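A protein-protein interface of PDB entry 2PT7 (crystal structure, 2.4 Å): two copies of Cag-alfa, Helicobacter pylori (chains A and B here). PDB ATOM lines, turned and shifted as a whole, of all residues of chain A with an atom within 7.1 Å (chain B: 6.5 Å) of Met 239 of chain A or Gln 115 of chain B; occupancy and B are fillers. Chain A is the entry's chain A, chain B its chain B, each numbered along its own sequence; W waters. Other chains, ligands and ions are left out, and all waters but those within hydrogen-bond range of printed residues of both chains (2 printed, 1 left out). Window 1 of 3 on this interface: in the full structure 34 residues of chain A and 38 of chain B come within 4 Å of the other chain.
Met 239 of chain A touches just these residues of chain B: Gln 115 (3.8 Å), Ser 129 (3.3 Å) and Ser 131 (3.5 Å). Of chain A, only Ser 235, Arg 238 and Met 239 come within 4 Å of Gln 115 of chain B. Printed residues of chain B within 4 Å of Arg 200 of chain A: Cys 49, Trp 65 and Ser 131. Printed residues of chain B within 4 Å of Ser 235 of chain A: Ile 103, Gln 115 and Val 117. Gln 220 of chain A touches none of the printed residues of chain B. The nearest residue of chain B that does not touch Met 239 of chain A is Cys 49 of chain B (4.1 Å). The nearest residue of chain A that does not touch Gln 115 of chain B is Lys 234 of chain A (5.3 Å).
O of Met 239 of chain A sits at hydrogen-bond distance from NE of Arg 200 of chain A (2.9 Å). The side-chain hydroxyl (OG) of Ser 235 of chain A is in hydrogen-bond range of the side-chain sulfur (SD) of Met 239 of chain A. OE1 of Gln 115 of chain B lies close to O of Leu 104 of chain B (3.5 Å). The backbone NH (N) of Arg 133 of chain B lies within hydrogen-bond range of the backbone carbonyl oxygen (O) of Arg 113 of chain B. The backbone carbonyl oxygen (O) of Gln 115 of chain B is in hydrogen-bond range of the backbone NH (N) of Ser 131 of chain B. N of Val 117 of chain B lies within hydrogen-bond range of O of Ser 129 of chain B (3.0 Å).
The guanidinium group (NH2) of Arg 200 of chain A sits close to the side-chain sulfur (SG) of Cys 49 of chain B (3.6 Å). The guanidinium group (NH2) of Arg 200 of chain A lies within hydrogen-bond range of the side-chain hydroxyl (OG) of Ser 131 of chain B (3.4 Å). OG of Ser 235 of chain A is in hydrogen-bond range of NE2 of Gln 115 of chain B, 3.1 Å away. The side-chain hydroxyl of Ser 105 of chain B lies within hydrogen-bond range of the guanidinium group of Arg 238 of chain A, 2.9 Å away. The guanidinium group (NE) of Arg 240 of chain A lies within salt-bridge range of the side-chain carboxylate (OE1) of Glu 47 of chain B. The indole nitrogen of Trp 65 of chain B lies within hydrogen-bond range of the side-chain carboxylate of Asp 242 of chain A (3.1 Å). The guanidinium group (NH2) of Arg 240 of chain A lies close to the guanidinium group (NE) of Arg 133 of chain B, 3.2 Å away.
Trp 65 of chain B touches Arg 200 of chain A (CZ2 to CD, 3.5 Å). Thr 219 of chain A touches Ser 129 of chain B. OG of Ser 235 of chain A touches CG2 of Ile 103 of chain B (3.6 Å). Val 117 of chain B touches Ser 235 of chain A (CG2 to OG, 3.5 Å). Arg 238 of chain A touches Gln 115 of chain B. Ser 131 of chain B touches Arg 238 of chain A (CB to O, 3.96 Å). Met 239 of chain A touches Gln 115 of chain B. Met 239 of chain A touches Ser 129 of chain B (CE to OG, 3.3 Å). Met 239 of chain A touches Ser 131 of chain B (CA to OG, 3.5 Å). Trp 65 of chain B touches Arg 240 of chain A (CZ2 to O, 3.7 Å).
No position is printed for both chains.
Printed residues of chain B that touch a printed residue of chain A: Glu 47, Cys 49, Trp 65, Ile 103, Ser 105, Gln 115, Val 117, Ser 129, Ser 131 and Arg 133. Hydrophobic or aromatic side chains of chain B within 4 Å of the printed part of chain A: Trp 65, Ile 103 and Val 117. Along chain A the printed residues that touch a printed residue of chain B span positions 200 to 242. Among the printed residues, Asp or Glu carboxylates within 4 Å of a Lys or Arg side-chain nitrogen of the other chain: Arg 240 of chain A with Glu 47 of chain B.
Water W1 lies within hydrogen-bond range of the side-chain hydroxyl of Ser 129 of chain B (2.5 Å), the side-chain hydroxyl of Thr 219 of chain A (2.7 Å) and the guanidinium group of Arg 200 of chain A (3.0 Å). Water W2 bridges OE2 of Glu 47 of chain B (2.6 Å) and O of Arg 238 of chain A (2.7 Å).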
ATOM      1  N   ARG A 200      -3.659  19.525 -19.279  1.00  0.00           N
ATOM      2  CA  ARG A 200      -3.847  20.538 -20.295  1.00  0.00           C
ATOM      3  C   ARG A 200      -3.814  19.851 -21.656  1.00  0.00           C
ATOM      4  O   ARG A 200      -2.797  19.262 -22.038  1.00  0.00           O
ATOM      5  CB  ARG A 200      -2.761  21.618 -20.174  1.00  0.00           C
ATOM      6  CG  ARG A 200      -2.714  22.634 -21.322  1.00  0.00           C
ATOM      7  CD  ARG A 200      -1.935  23.873 -20.924  1.00  0.00           C
ATOM      8  NE  ARG A 200      -1.587  24.727 -22.062  1.00  0.00           N
ATOM      9  CZ  ARG A 200      -2.368  25.676 -22.580  1.00  0.00           C
ATOM     10  NH1 ARG A 200      -3.578  25.896 -22.081  1.00  0.00           N
ATOM     11  NH2 ARG A 200      -1.949  26.396 -23.620  1.00  0.00           N
ATOM     12  N   ILE A 202      -4.221  20.000 -25.850  1.00  0.00           N
ATOM     13  CA  ILE A 202      -4.237  20.794 -27.068  1.00  0.00           C
ATOM     14  C   ILE A 202      -4.602  19.883 -28.233  1.00  0.00           C
ATOM     15  O   ILE A 202      -3.928  18.880 -28.495  1.00  0.00           O
ATOM     16  CB  ILE A 202      -2.911  21.566 -27.291  1.00  0.00           C
ATOM     17  CG1 ILE A 202      -2.745  22.629 -26.196  1.00  0.00           C
ATOM     18  CG2 ILE A 202      -2.878  22.214 -28.695  1.00  0.00           C
ATOM     19  CD1 ILE A 202      -1.414  23.292 -26.171  1.00  0.00           C
ATOM     20  N   THR A 219      -6.820  24.117 -25.390  1.00  0.00           N
ATOM     21  CA  THR A 219      -6.833  25.007 -26.549  1.00  0.00           C
ATOM     22  C   THR A 219      -6.966  24.187 -27.840  1.00  0.00           C
ATOM     23  O   THR A 219      -6.249  23.207 -28.045  1.00  0.00           O
ATOM     24  CB  THR A 219      -5.583  25.928 -26.604  1.00  0.00           C
ATOM     25  OG1 THR A 219      -5.615  26.849 -25.504  1.00  0.00           O
ATOM     26  CG2 THR A 219      -5.556  26.727 -27.898  1.00  0.00           C
ATOM     27  N   GLN A 220      -7.910  24.598 -28.686  1.00  0.00           N
ATOM     28  CA  GLN A 220      -8.120  24.000 -30.003  1.00  0.00           C
ATOM     29  C   GLN A 220      -7.360  24.766 -31.077  1.00  0.00           C
ATOM     30  O   GLN A 220      -7.484  25.998 -31.193  1.00  0.00           O
ATOM     31  CB  GLN A 220      -9.605  24.005 -30.364  1.00  0.00           C
ATOM     32  CG  GLN A 220     -10.503  23.238 -29.417  1.00  0.00           C
ATOM     33  CD  GLN A 220     -11.895  23.834 -29.339  1.00  0.00           C
ATOM     34  OE1 GLN A 220     -12.113  24.864 -28.688  1.00  0.00           O
ATOM     35  NE2 GLN A 220     -12.851  23.182 -29.990  1.00  0.00           N
ATOM     36  N   LEU A 221      -6.585  24.029 -31.871  1.00  0.00           N
ATOM     37  CA  LEU A 221      -5.853  24.612 -32.993  1.00  0.00           C
ATOM     38  C   LEU A 221      -6.401  24.077 -34.310  1.00  0.00           C
ATOM     39  O   LEU A 221      -6.734  22.889 -34.424  1.00  0.00           O
ATOM     40  CB  LEU A 221      -4.350  24.331 -32.890  1.00  0.00           C
ATOM     41  CG  LEU A 221      -3.581  24.768 -31.634  1.00  0.00           C
ATOM     42  CD1 LEU A 221      -2.132  24.335 -31.742  1.00  0.00           C
ATOM     43  CD2 LEU A 221      -3.665  26.259 -31.414  1.00  0.00           C
ATOM     44  N   ASP A 231       2.418  23.312 -38.788  1.00  0.00           N
ATOM     45  CA  ASP A 231       2.483  24.648 -38.179  1.00  0.00           C
ATOM     46  C   ASP A 231       1.787  24.669 -36.819  1.00  0.00           C
ATOM     47  O   ASP A 231       2.255  25.337 -35.894  1.00  0.00           O
ATOM     48  CB  ASP A 231       1.828  25.707 -39.076  1.00  0.00           C
ATOM     49  CG  ASP A 231       2.629  25.999 -40.333  1.00  0.00           C
ATOM     50  OD1 ASP A 231       3.868  25.810 -40.314  1.00  0.00           O
ATOM     51  OD2 ASP A 231       2.016  26.425 -41.345  1.00  0.00           O
ATOM     52  N   CYS A 232       0.661  23.963 -36.714  1.00  0.00           N
ATOM     53  CA  CYS A 232      -0.104  23.878 -35.468  1.00  0.00           C
ATOM     54  C   CYS A 232       0.616  23.007 -34.446  1.00  0.00           C
ATOM     55  O   CYS A 232       0.579  23.292 -33.259  1.00  0.00           O
ATOM     56  CB  CYS A 232      -1.513  23.316 -35.727  1.00  0.00           C
ATOM     57  SG  CYS A 232      -2.595  24.385 -36.705  1.00  0.00           S
ATOM     58  N   LYS A 234       3.932  22.518 -34.327  1.00  0.00           N
ATOM     59  CA  LYS A 234       5.068  23.348 -33.916  1.00  0.00           C
ATOM     60  C   LYS A 234       4.668  24.370 -32.848  1.00  0.00           C
ATOM     61  O   LYS A 234       5.387  24.580 -31.873  1.00  0.00           O
ATOM     62  CB  LYS A 234       5.652  24.050 -35.143  1.00  0.00           C
ATOM     63  CG  LYS A 234       6.747  25.051 -34.856  1.00  0.00           C
ATOM     64  CD  LYS A 234       7.492  25.357 -36.138  1.00  0.00           C
ATOM     65  CE  LYS A 234       8.327  26.606 -36.013  1.00  0.00           C
ATOM     66  NZ  LYS A 234       7.488  27.779 -36.319  1.00  0.00           N
ATOM     67  N   SER A 235       3.511  24.998 -33.046  1.00  0.00           N
ATOM     68  CA  SER A 235       2.973  25.963 -32.091  1.00  0.00           C
ATOM     69  C   SER A 235       2.570  25.271 -30.790  1.00  0.00           C
ATOM     70  O   SER A 235       2.873  25.753 -29.705  1.00  0.00           O
ATOM     71  CB  SER A 235       1.772  26.683 -32.698  1.00  0.00           C
ATOM     72  OG  SER A 235       1.257  27.638 -31.800  1.00  0.00           O
ATOM     73  N   CYS A 236       1.899  24.133 -30.934  1.00  0.00           N
ATOM     74  CA  CYS A 236       1.460  23.292 -29.826  1.00  0.00           C
ATOM     75  C   CYS A 236       2.575  23.002 -28.816  1.00  0.00           C
ATOM     76  O   CYS A 236       2.338  23.050 -27.607  1.00  0.00           O
ATOM     77  CB  CYS A 236       0.870  21.989 -30.391  1.00  0.00           C
ATOM     78  SG  CYS A 236       0.404  20.741 -29.207  1.00  0.00           S
ATOM     79  N   LEU A 237       3.778  22.714 -29.316  1.00  0.00           N
ATOM     80  CA  LEU A 237       4.939  22.365 -28.485  1.00  0.00           C
ATOM     81  C   LEU A 237       5.465  23.546 -27.689  1.00  0.00           C
ATOM     82  O   LEU A 237       6.234  23.374 -26.746  1.00  0.00           O
ATOM     83  CB  LEU A 237       6.068  21.755 -29.337  1.00  0.00           C
ATOM     84  CG  LEU A 237       5.828  20.376 -29.976  1.00  0.00           C
ATOM     85  CD1 LEU A 237       6.992  19.973 -30.890  1.00  0.00           C
ATOM     86  CD2 LEU A 237       5.572  19.291 -28.930  1.00  0.00           C
ATOM     87  N   ARG A 238       5.042  24.746 -28.080  1.00  0.00           N
ATOM     88  CA  ARG A 238       5.431  25.985 -27.411  1.00  0.00           C
ATOM     89  C   ARG A 238       4.336  26.490 -26.467  1.00  0.00           C
ATOM     90  O   ARG A 238       4.436  27.594 -25.914  1.00  0.00           O
ATOM     91  CB  ARG A 238       5.781  27.031 -28.467  1.00  0.00           C
ATOM     92  CG  ARG A 238       6.985  26.631 -29.306  1.00  0.00           C
ATOM     93  CD  ARG A 238       7.156  27.469 -30.564  1.00  0.00           C
ATOM     94  NE  ARG A 238       8.346  27.021 -31.294  1.00  0.00           N
ATOM     95  CZ  ARG A 238       9.025  27.750 -32.180  1.00  0.00           C
ATOM     96  NH1 ARG A 238       8.651  28.991 -32.478  1.00  0.00           N
ATOM     97  NH2 ARG A 238      10.100  27.235 -32.766  1.00  0.00           N
ATOM     98  N   MET A 239       3.311  25.659 -26.272  1.00  0.00           N
ATOM     99  CA  MET A 239       2.112  26.025 -25.503  1.00  0.00           C
ATOM    100  C   MET A 239       1.921  25.210 -24.219  1.00  0.00           C
ATOM    101  O   MET A 239       0.835  25.219 -23.636  1.00  0.00           O
ATOM    102  CB  MET A 239       0.862  25.922 -26.396  1.00  0.00           C
ATOM    103  CG  MET A 239       0.854  26.898 -27.567  1.00  0.00           C
ATOM    104  SD  MET A 239      -0.299  26.462 -28.874  1.00  0.00           S
ATOM    105  CE  MET A 239      -1.849  26.987 -28.128  1.00  0.00           C
ATOM    106  N   ARG A 240       2.981  24.516 -23.795  1.00  0.00           N
ATOM    107  CA  ARG A 240       2.995  23.660 -22.597  1.00  0.00           C
ATOM    108  C   ARG A 240       1.801  22.687 -22.459  1.00  0.00           C
ATOM    109  O   ARG A 240       1.075  22.730 -21.459  1.00  0.00           O
ATOM    110  CB  ARG A 240       3.179  24.504 -21.324  1.00  0.00           C
ATOM    111  CG  ARG A 240       3.490  23.719 -20.049  1.00  0.00           C
ATOM    112  CD  ARG A 240       4.922  23.181 -19.997  1.00  0.00           C
ATOM    113  NE  ARG A 240       5.850  24.242 -19.646  1.00  0.00           N
ATOM    114  CZ  ARG A 240       6.534  24.331 -18.510  1.00  0.00           C
ATOM    115  NH1 ARG A 240       6.461  23.395 -17.572  1.00  0.00           N
ATOM    116  NH2 ARG A 240       7.319  25.379 -18.330  1.00  0.00           N
ATOM    117  N   PRO A 241       1.612  21.789 -23.446  1.00  0.00           N
ATOM    118  CA  PRO A 241       0.531  20.812 -23.294  1.00  0.00           C
ATOM    119  C   PRO A 241       0.941  19.601 -22.449  1.00  0.00           C
ATOM    120  O   PRO A 241       2.122  19.259 -22.394  1.00  0.00           O
ATOM    121  CB  PRO A 241       0.269  20.363 -24.734  1.00  0.00           C
ATOM    122  CG  PRO A 241       1.583  20.512 -25.427  1.00  0.00           C
ATOM    123  CD  PRO A 241       2.349  21.610 -24.716  1.00  0.00           C
ATOM    124  N   ASP A 242      -0.033  18.959 -21.811  1.00  0.00           N
ATOM    125  CA  ASP A 242       0.183  17.654 -21.191  1.00  0.00           C
ATOM    126  C   ASP A 242      -0.211  16.571 -22.182  1.00  0.00           C
ATOM    127  O   ASP A 242       0.413  15.506 -22.248  1.00  0.00           O
ATOM    128  CB  ASP A 242      -0.644  17.507 -19.911  1.00  0.00           C
ATOM    129  CG  ASP A 242      -0.253  18.510 -18.840  1.00  0.00           C
ATOM    130  OD1 ASP A 242       0.960  18.635 -18.554  1.00  0.00           O
ATOM    131  OD2 ASP A 242      -1.157  19.167 -18.283  1.00  0.00           O
ATOM    132  N   GLU B  47       4.707  28.231 -15.839  1.00  0.00           N
ATOM    133  CA  GLU B  47       3.905  28.571 -17.010  1.00  0.00           C
ATOM    134  C   GLU B  47       2.651  29.382 -16.661  1.00  0.00           C
ATOM    135  O   GLU B  47       1.977  29.107 -15.670  1.00  0.00           O
ATOM    136  CB  GLU B  47       3.497  27.290 -17.760  1.00  0.00           C
ATOM    137  CG  GLU B  47       2.962  27.510 -19.175  1.00  0.00           C
ATOM    138  CD  GLU B  47       4.058  27.648 -20.219  1.00  0.00           C
ATOM    139  OE1 GLU B  47       5.231  27.316 -19.926  1.00  0.00           O
ATOM    140  OE2 GLU B  47       3.737  28.066 -21.356  1.00  0.00           O
ATOM    141  N   CYS B  49      -0.888  30.477 -18.722  1.00  0.00           N
ATOM    142  CA  CYS B  49      -1.687  30.261 -19.932  1.00  0.00           C
ATOM    143  C   CYS B  49      -3.053  30.937 -19.894  1.00  0.00           C
ATOM    144  O   CYS B  49      -3.711  30.983 -18.851  1.00  0.00           O
ATOM    145  CB  CYS B  49      -1.875  28.766 -20.203  1.00  0.00           C
ATOM    146  SG  CYS B  49      -0.384  27.920 -20.764  1.00  0.00           S
ATOM    147  N   TRP B  65      -1.798  22.575 -12.131  1.00  0.00           N
ATOM    148  CA  TRP B  65      -2.430  23.694 -12.823  1.00  0.00           C
ATOM    149  C   TRP B  65      -3.454  24.326 -11.900  1.00  0.00           C
ATOM    150  O   TRP B  65      -4.295  23.628 -11.332  1.00  0.00           O
ATOM    151  CB  TRP B  65      -3.122  23.233 -14.108  1.00  0.00           C
ATOM    152  CG  TRP B  65      -2.188  22.926 -15.243  1.00  0.00           C
ATOM    153  CD1 TRP B  65      -1.768  21.695 -15.644  1.00  0.00           C
ATOM    154  CD2 TRP B  65      -1.563  23.871 -16.124  1.00  0.00           C
ATOM    155  NE1 TRP B  65      -0.924  21.810 -16.721  1.00  0.00           N
ATOM    156  CE2 TRP B  65      -0.779  23.134 -17.037  1.00  0.00           C
ATOM    157  CE3 TRP B  65      -1.595  25.269 -16.231  1.00  0.00           C
ATOM    158  CZ2 TRP B  65      -0.026  23.746 -18.050  1.00  0.00           C
ATOM    159  CZ3 TRP B  65      -0.845  25.880 -17.239  1.00  0.00           C
ATOM    160  CH2 TRP B  65      -0.070  25.115 -18.134  1.00  0.00           C
ATOM    161  N   ILE B 103      -0.028  33.146 -35.817  1.00  0.00           N
ATOM    162  CA  ILE B 103       0.808  32.457 -34.825  1.00  0.00           C
ATOM    163  C   ILE B 103       2.071  33.269 -34.555  1.00  0.00           C
ATOM    164  O   ILE B 103       2.794  33.651 -35.484  1.00  0.00           O
ATOM    165  CB  ILE B 103       1.196  31.015 -35.283  1.00  0.00           C
ATOM    166  CG1 ILE B 103      -0.049  30.225 -35.714  1.00  0.00           C
ATOM    167  CG2 ILE B 103       1.986  30.270 -34.180  1.00  0.00           C
ATOM    168  CD1 ILE B 103       0.245  28.853 -36.283  1.00  0.00           C
ATOM    169  N   LEU B 104       2.331  33.530 -33.278  1.00  0.00           N
ATOM    170  CA  LEU B 104       3.475  34.332 -32.874  1.00  0.00           C
ATOM    171  C   LEU B 104       4.288  33.671 -31.767  1.00  0.00           C
ATOM    172  O   LEU B 104       3.729  33.197 -30.782  1.00  0.00           O
ATOM    173  CB  LEU B 104       3.013  35.724 -32.423  1.00  0.00           C
ATOM    174  CG  LEU B 104       4.038  36.720 -31.860  1.00  0.00           C
ATOM    175  CD1 LEU B 104       4.881  37.330 -32.962  1.00  0.00           C
ATOM    176  CD2 LEU B 104       3.325  37.809 -31.071  1.00  0.00           C
ATOM    177  N   SER B 105       5.607  33.642 -31.954  1.00  0.00           N
ATOM    178  CA  SER B 105       6.551  33.340 -30.890  1.00  0.00           C
ATOM    179  C   SER B 105       7.373  34.597 -30.626  1.00  0.00           C
ATOM    180  O   SER B 105       8.047  35.107 -31.524  1.00  0.00           O
ATOM    181  CB  SER B 105       7.475  32.181 -31.285  1.00  0.00           C
ATOM    182  OG  SER B 105       6.723  31.067 -31.721  1.00  0.00           O
ATOM    183  N   SER B 106       7.308  35.094 -29.396  1.00  0.00           N
ATOM    184  CA  SER B 106       7.966  36.342 -29.031  1.00  0.00           C
ATOM    185  C   SER B 106       8.398  36.323 -27.565  1.00  0.00           C
ATOM    186  O   SER B 106       8.518  35.256 -26.967  1.00  0.00           O
ATOM    187  CB  SER B 106       7.043  37.533 -29.322  1.00  0.00           C
ATOM    188  OG  SER B 106       7.768  38.745 -29.382  1.00  0.00           O
ATOM    189  N   ARG B 113       9.459  33.825 -22.633  1.00  0.00           N
ATOM    190  CA  ARG B 113       8.871  33.397 -23.908  1.00  0.00           C
ATOM    191  C   ARG B 113       7.354  33.461 -23.943  1.00  0.00           C
ATOM    192  O   ARG B 113       6.683  33.058 -22.994  1.00  0.00           O
ATOM    193  CB  ARG B 113       9.322  31.970 -24.236  1.00  0.00           C
ATOM    194  CG  ARG B 113      10.620  31.902 -25.010  1.00  0.00           C
ATOM    195  CD  ARG B 113      11.161  30.494 -25.034  1.00  0.00           C
ATOM    196  NE  ARG B 113      12.330  30.376 -24.173  1.00  0.00           N
ATOM    197  CZ  ARG B 113      13.585  30.382 -24.613  1.00  0.00           C
ATOM    198  NH1 ARG B 113      13.840  30.482 -25.913  1.00  0.00           N
ATOM    199  NH2 ARG B 113      14.587  30.274 -23.754  1.00  0.00           N
ATOM    200  N   VAL B 114       6.827  33.953 -25.060  1.00  0.00           N
ATOM    201  CA  VAL B 114       5.383  34.092 -25.261  1.00  0.00           C
ATOM    202  C   VAL B 114       4.960  33.477 -26.591  1.00  0.00           C
ATOM    203  O   VAL B 114       5.460  33.858 -27.648  1.00  0.00           O
ATOM    204  CB  VAL B 114       4.904  35.574 -25.239  1.00  0.00           C
ATOM    205  CG1 VAL B 114       3.426  35.651 -24.881  1.00  0.00           C
ATOM    206  CG2 VAL B 114       5.702  36.384 -24.270  1.00  0.00           C
ATOM    207  N   GLN B 115       4.029  32.532 -26.515  1.00  0.00           N
ATOM    208  CA  GLN B 115       3.367  31.978 -27.677  1.00  0.00           C
ATOM    209  C   GLN B 115       1.940  32.538 -27.754  1.00  0.00           C
ATOM    210  O   GLN B 115       1.142  32.341 -26.832  1.00  0.00           O
ATOM    211  CB  GLN B 115       3.334  30.447 -27.590  1.00  0.00           C
ATOM    212  CG  GLN B 115       2.912  29.753 -28.876  1.00  0.00           C
ATOM    213  CD  GLN B 115       3.967  29.854 -29.965  1.00  0.00           C
ATOM    214  OE1 GLN B 115       5.122  30.184 -29.694  1.00  0.00           O
ATOM    215  NE2 GLN B 115       3.576  29.562 -31.201  1.00  0.00           N
ATOM    216  N   ILE B 116       1.635  33.246 -28.841  1.00  0.00           N
ATOM    217  CA  ILE B 116       0.299  33.791 -29.047  1.00  0.00           C
ATOM    218  C   ILE B 116      -0.310  33.246 -30.347  1.00  0.00           C
ATOM    219  O   ILE B 116       0.347  33.207 -31.393  1.00  0.00           O
ATOM    220  CB  ILE B 116       0.257  35.353 -29.014  1.00  0.00           C
ATOM    221  CG1 ILE B 116       1.070  35.898 -27.826  1.00  0.00           C
ATOM    222  CG2 ILE B 116      -1.206  35.847 -28.983  1.00  0.00           C
ATOM    223  CD1 ILE B 116       0.991  37.417 -27.597  1.00  0.00           C
ATOM    224  N   VAL B 117      -1.565  32.807 -30.253  1.00  0.00           N
ATOM    225  CA  VAL B 117      -2.300  32.261 -31.384  1.00  0.00           C
ATOM    226  C   VAL B 117      -3.647  32.977 -31.490  1.00  0.00           C
ATOM    227  O   VAL B 117      -4.349  33.155 -30.489  1.00  0.00           O
ATOM    228  CB  VAL B 117      -2.507  30.722 -31.267  1.00  0.00           C
ATOM    229  CG1 VAL B 117      -3.102  30.168 -32.544  1.00  0.00           C
ATOM    230  CG2 VAL B 117      -1.188  30.007 -30.974  1.00  0.00           C
ATOM    231  N   SER B 129      -5.267  32.712 -27.679  1.00  0.00           N
ATOM    232  CA  SER B 129      -4.448  31.817 -26.866  1.00  0.00           C
ATOM    233  C   SER B 129      -3.097  32.462 -26.523  1.00  0.00           C
ATOM    234  O   SER B 129      -2.380  32.906 -27.416  1.00  0.00           O
ATOM    235  CB  SER B 129      -4.232  30.503 -27.617  1.00  0.00           C
ATOM    236  OG  SER B 129      -3.246  29.704 -26.986  1.00  0.00           O
ATOM    237  N   ILE B 130      -2.763  32.519 -25.234  1.00  0.00           N
ATOM    238  CA  ILE B 130      -1.467  33.045 -24.784  1.00  0.00           C
ATOM    239  C   ILE B 130      -0.771  32.053 -23.857  1.00  0.00           C
ATOM    240  O   ILE B 130      -1.363  31.592 -22.878  1.00  0.00           O
ATOM    241  CB  ILE B 130      -1.613  34.430 -24.070  1.00  0.00           C
ATOM    242  CG1 ILE B 130      -2.132  35.499 -25.045  1.00  0.00           C
ATOM    243  CG2 ILE B 130      -0.265  34.888 -23.463  1.00  0.00           C
ATOM    244  CD1 ILE B 130      -2.885  36.637 -24.373  1.00  0.00           C
ATOM    245  N   SER B 131       0.487  31.729 -24.161  1.00  0.00           N
ATOM    246  CA  SER B 131       1.286  30.839 -23.309  1.00  0.00           C
ATOM    247  C   SER B 131       2.614  31.483 -22.947  1.00  0.00           C
ATOM    248  O   SER B 131       3.432  31.757 -23.823  1.00  0.00           O
ATOM    249  CB  SER B 131       1.534  29.488 -23.991  1.00  0.00           C
ATOM    250  OG  SER B 131       0.316  28.843 -24.324  1.00  0.00           O
ATOM    251  N   ILE B 132       2.824  31.723 -21.651  1.00  0.00           N
ATOM    252  CA  ILE B 132       4.055  32.365 -21.185  1.00  0.00           C
ATOM    253  C   ILE B 132       4.901  31.393 -20.381  1.00  0.00           C
ATOM    254  O   ILE B 132       4.447  30.855 -19.371  1.00  0.00           O
ATOM    255  CB  ILE B 132       3.798  33.659 -20.354  1.00  0.00           C
ATOM    256  CG1 ILE B 132       2.785  34.574 -21.046  1.00  0.00           C
ATOM    257  CG2 ILE B 132       5.126  34.418 -20.085  1.00  0.00           C
ATOM    258  CD1 ILE B 132       2.200  35.656 -20.137  1.00  0.00           C
ATOM    259  N   ARG B 133       6.134  31.181 -20.838  1.00  0.00           N
ATOM    260  CA  ARG B 133       7.076  30.288 -20.178  1.00  0.00           C
ATOM    261  C   ARG B 133       7.883  31.062 -19.141  1.00  0.00           C
ATOM    262  O   ARG B 133       8.577  32.024 -19.471  1.00  0.00           O
ATOM    263  CB  ARG B 133       7.995  29.618 -21.217  1.00  0.00           C
ATOM    264  CG  ARG B 133       9.196  28.837 -20.658  1.00  0.00           C
ATOM    265  CD  ARG B 133       8.791  27.718 -19.705  1.00  0.00           C
ATOM    266  NE  ARG B 133       9.914  26.827 -19.382  1.00  0.00           N
ATOM    267  CZ  ARG B 133      10.342  26.561 -18.148  1.00  0.00           C
ATOM    268  NH1 ARG B 133       9.738  27.105 -17.101  1.00  0.00           N
ATOM    269  NH2 ARG B 133      11.363  25.734 -17.954  1.00  0.00           N
HETATM  270  O   HOH W   1      -3.637  28.596 -24.820  1.00  0.00           O
HETATM  271  O   HOH W   2       5.251  28.284 -23.475  1.00  0.00           O
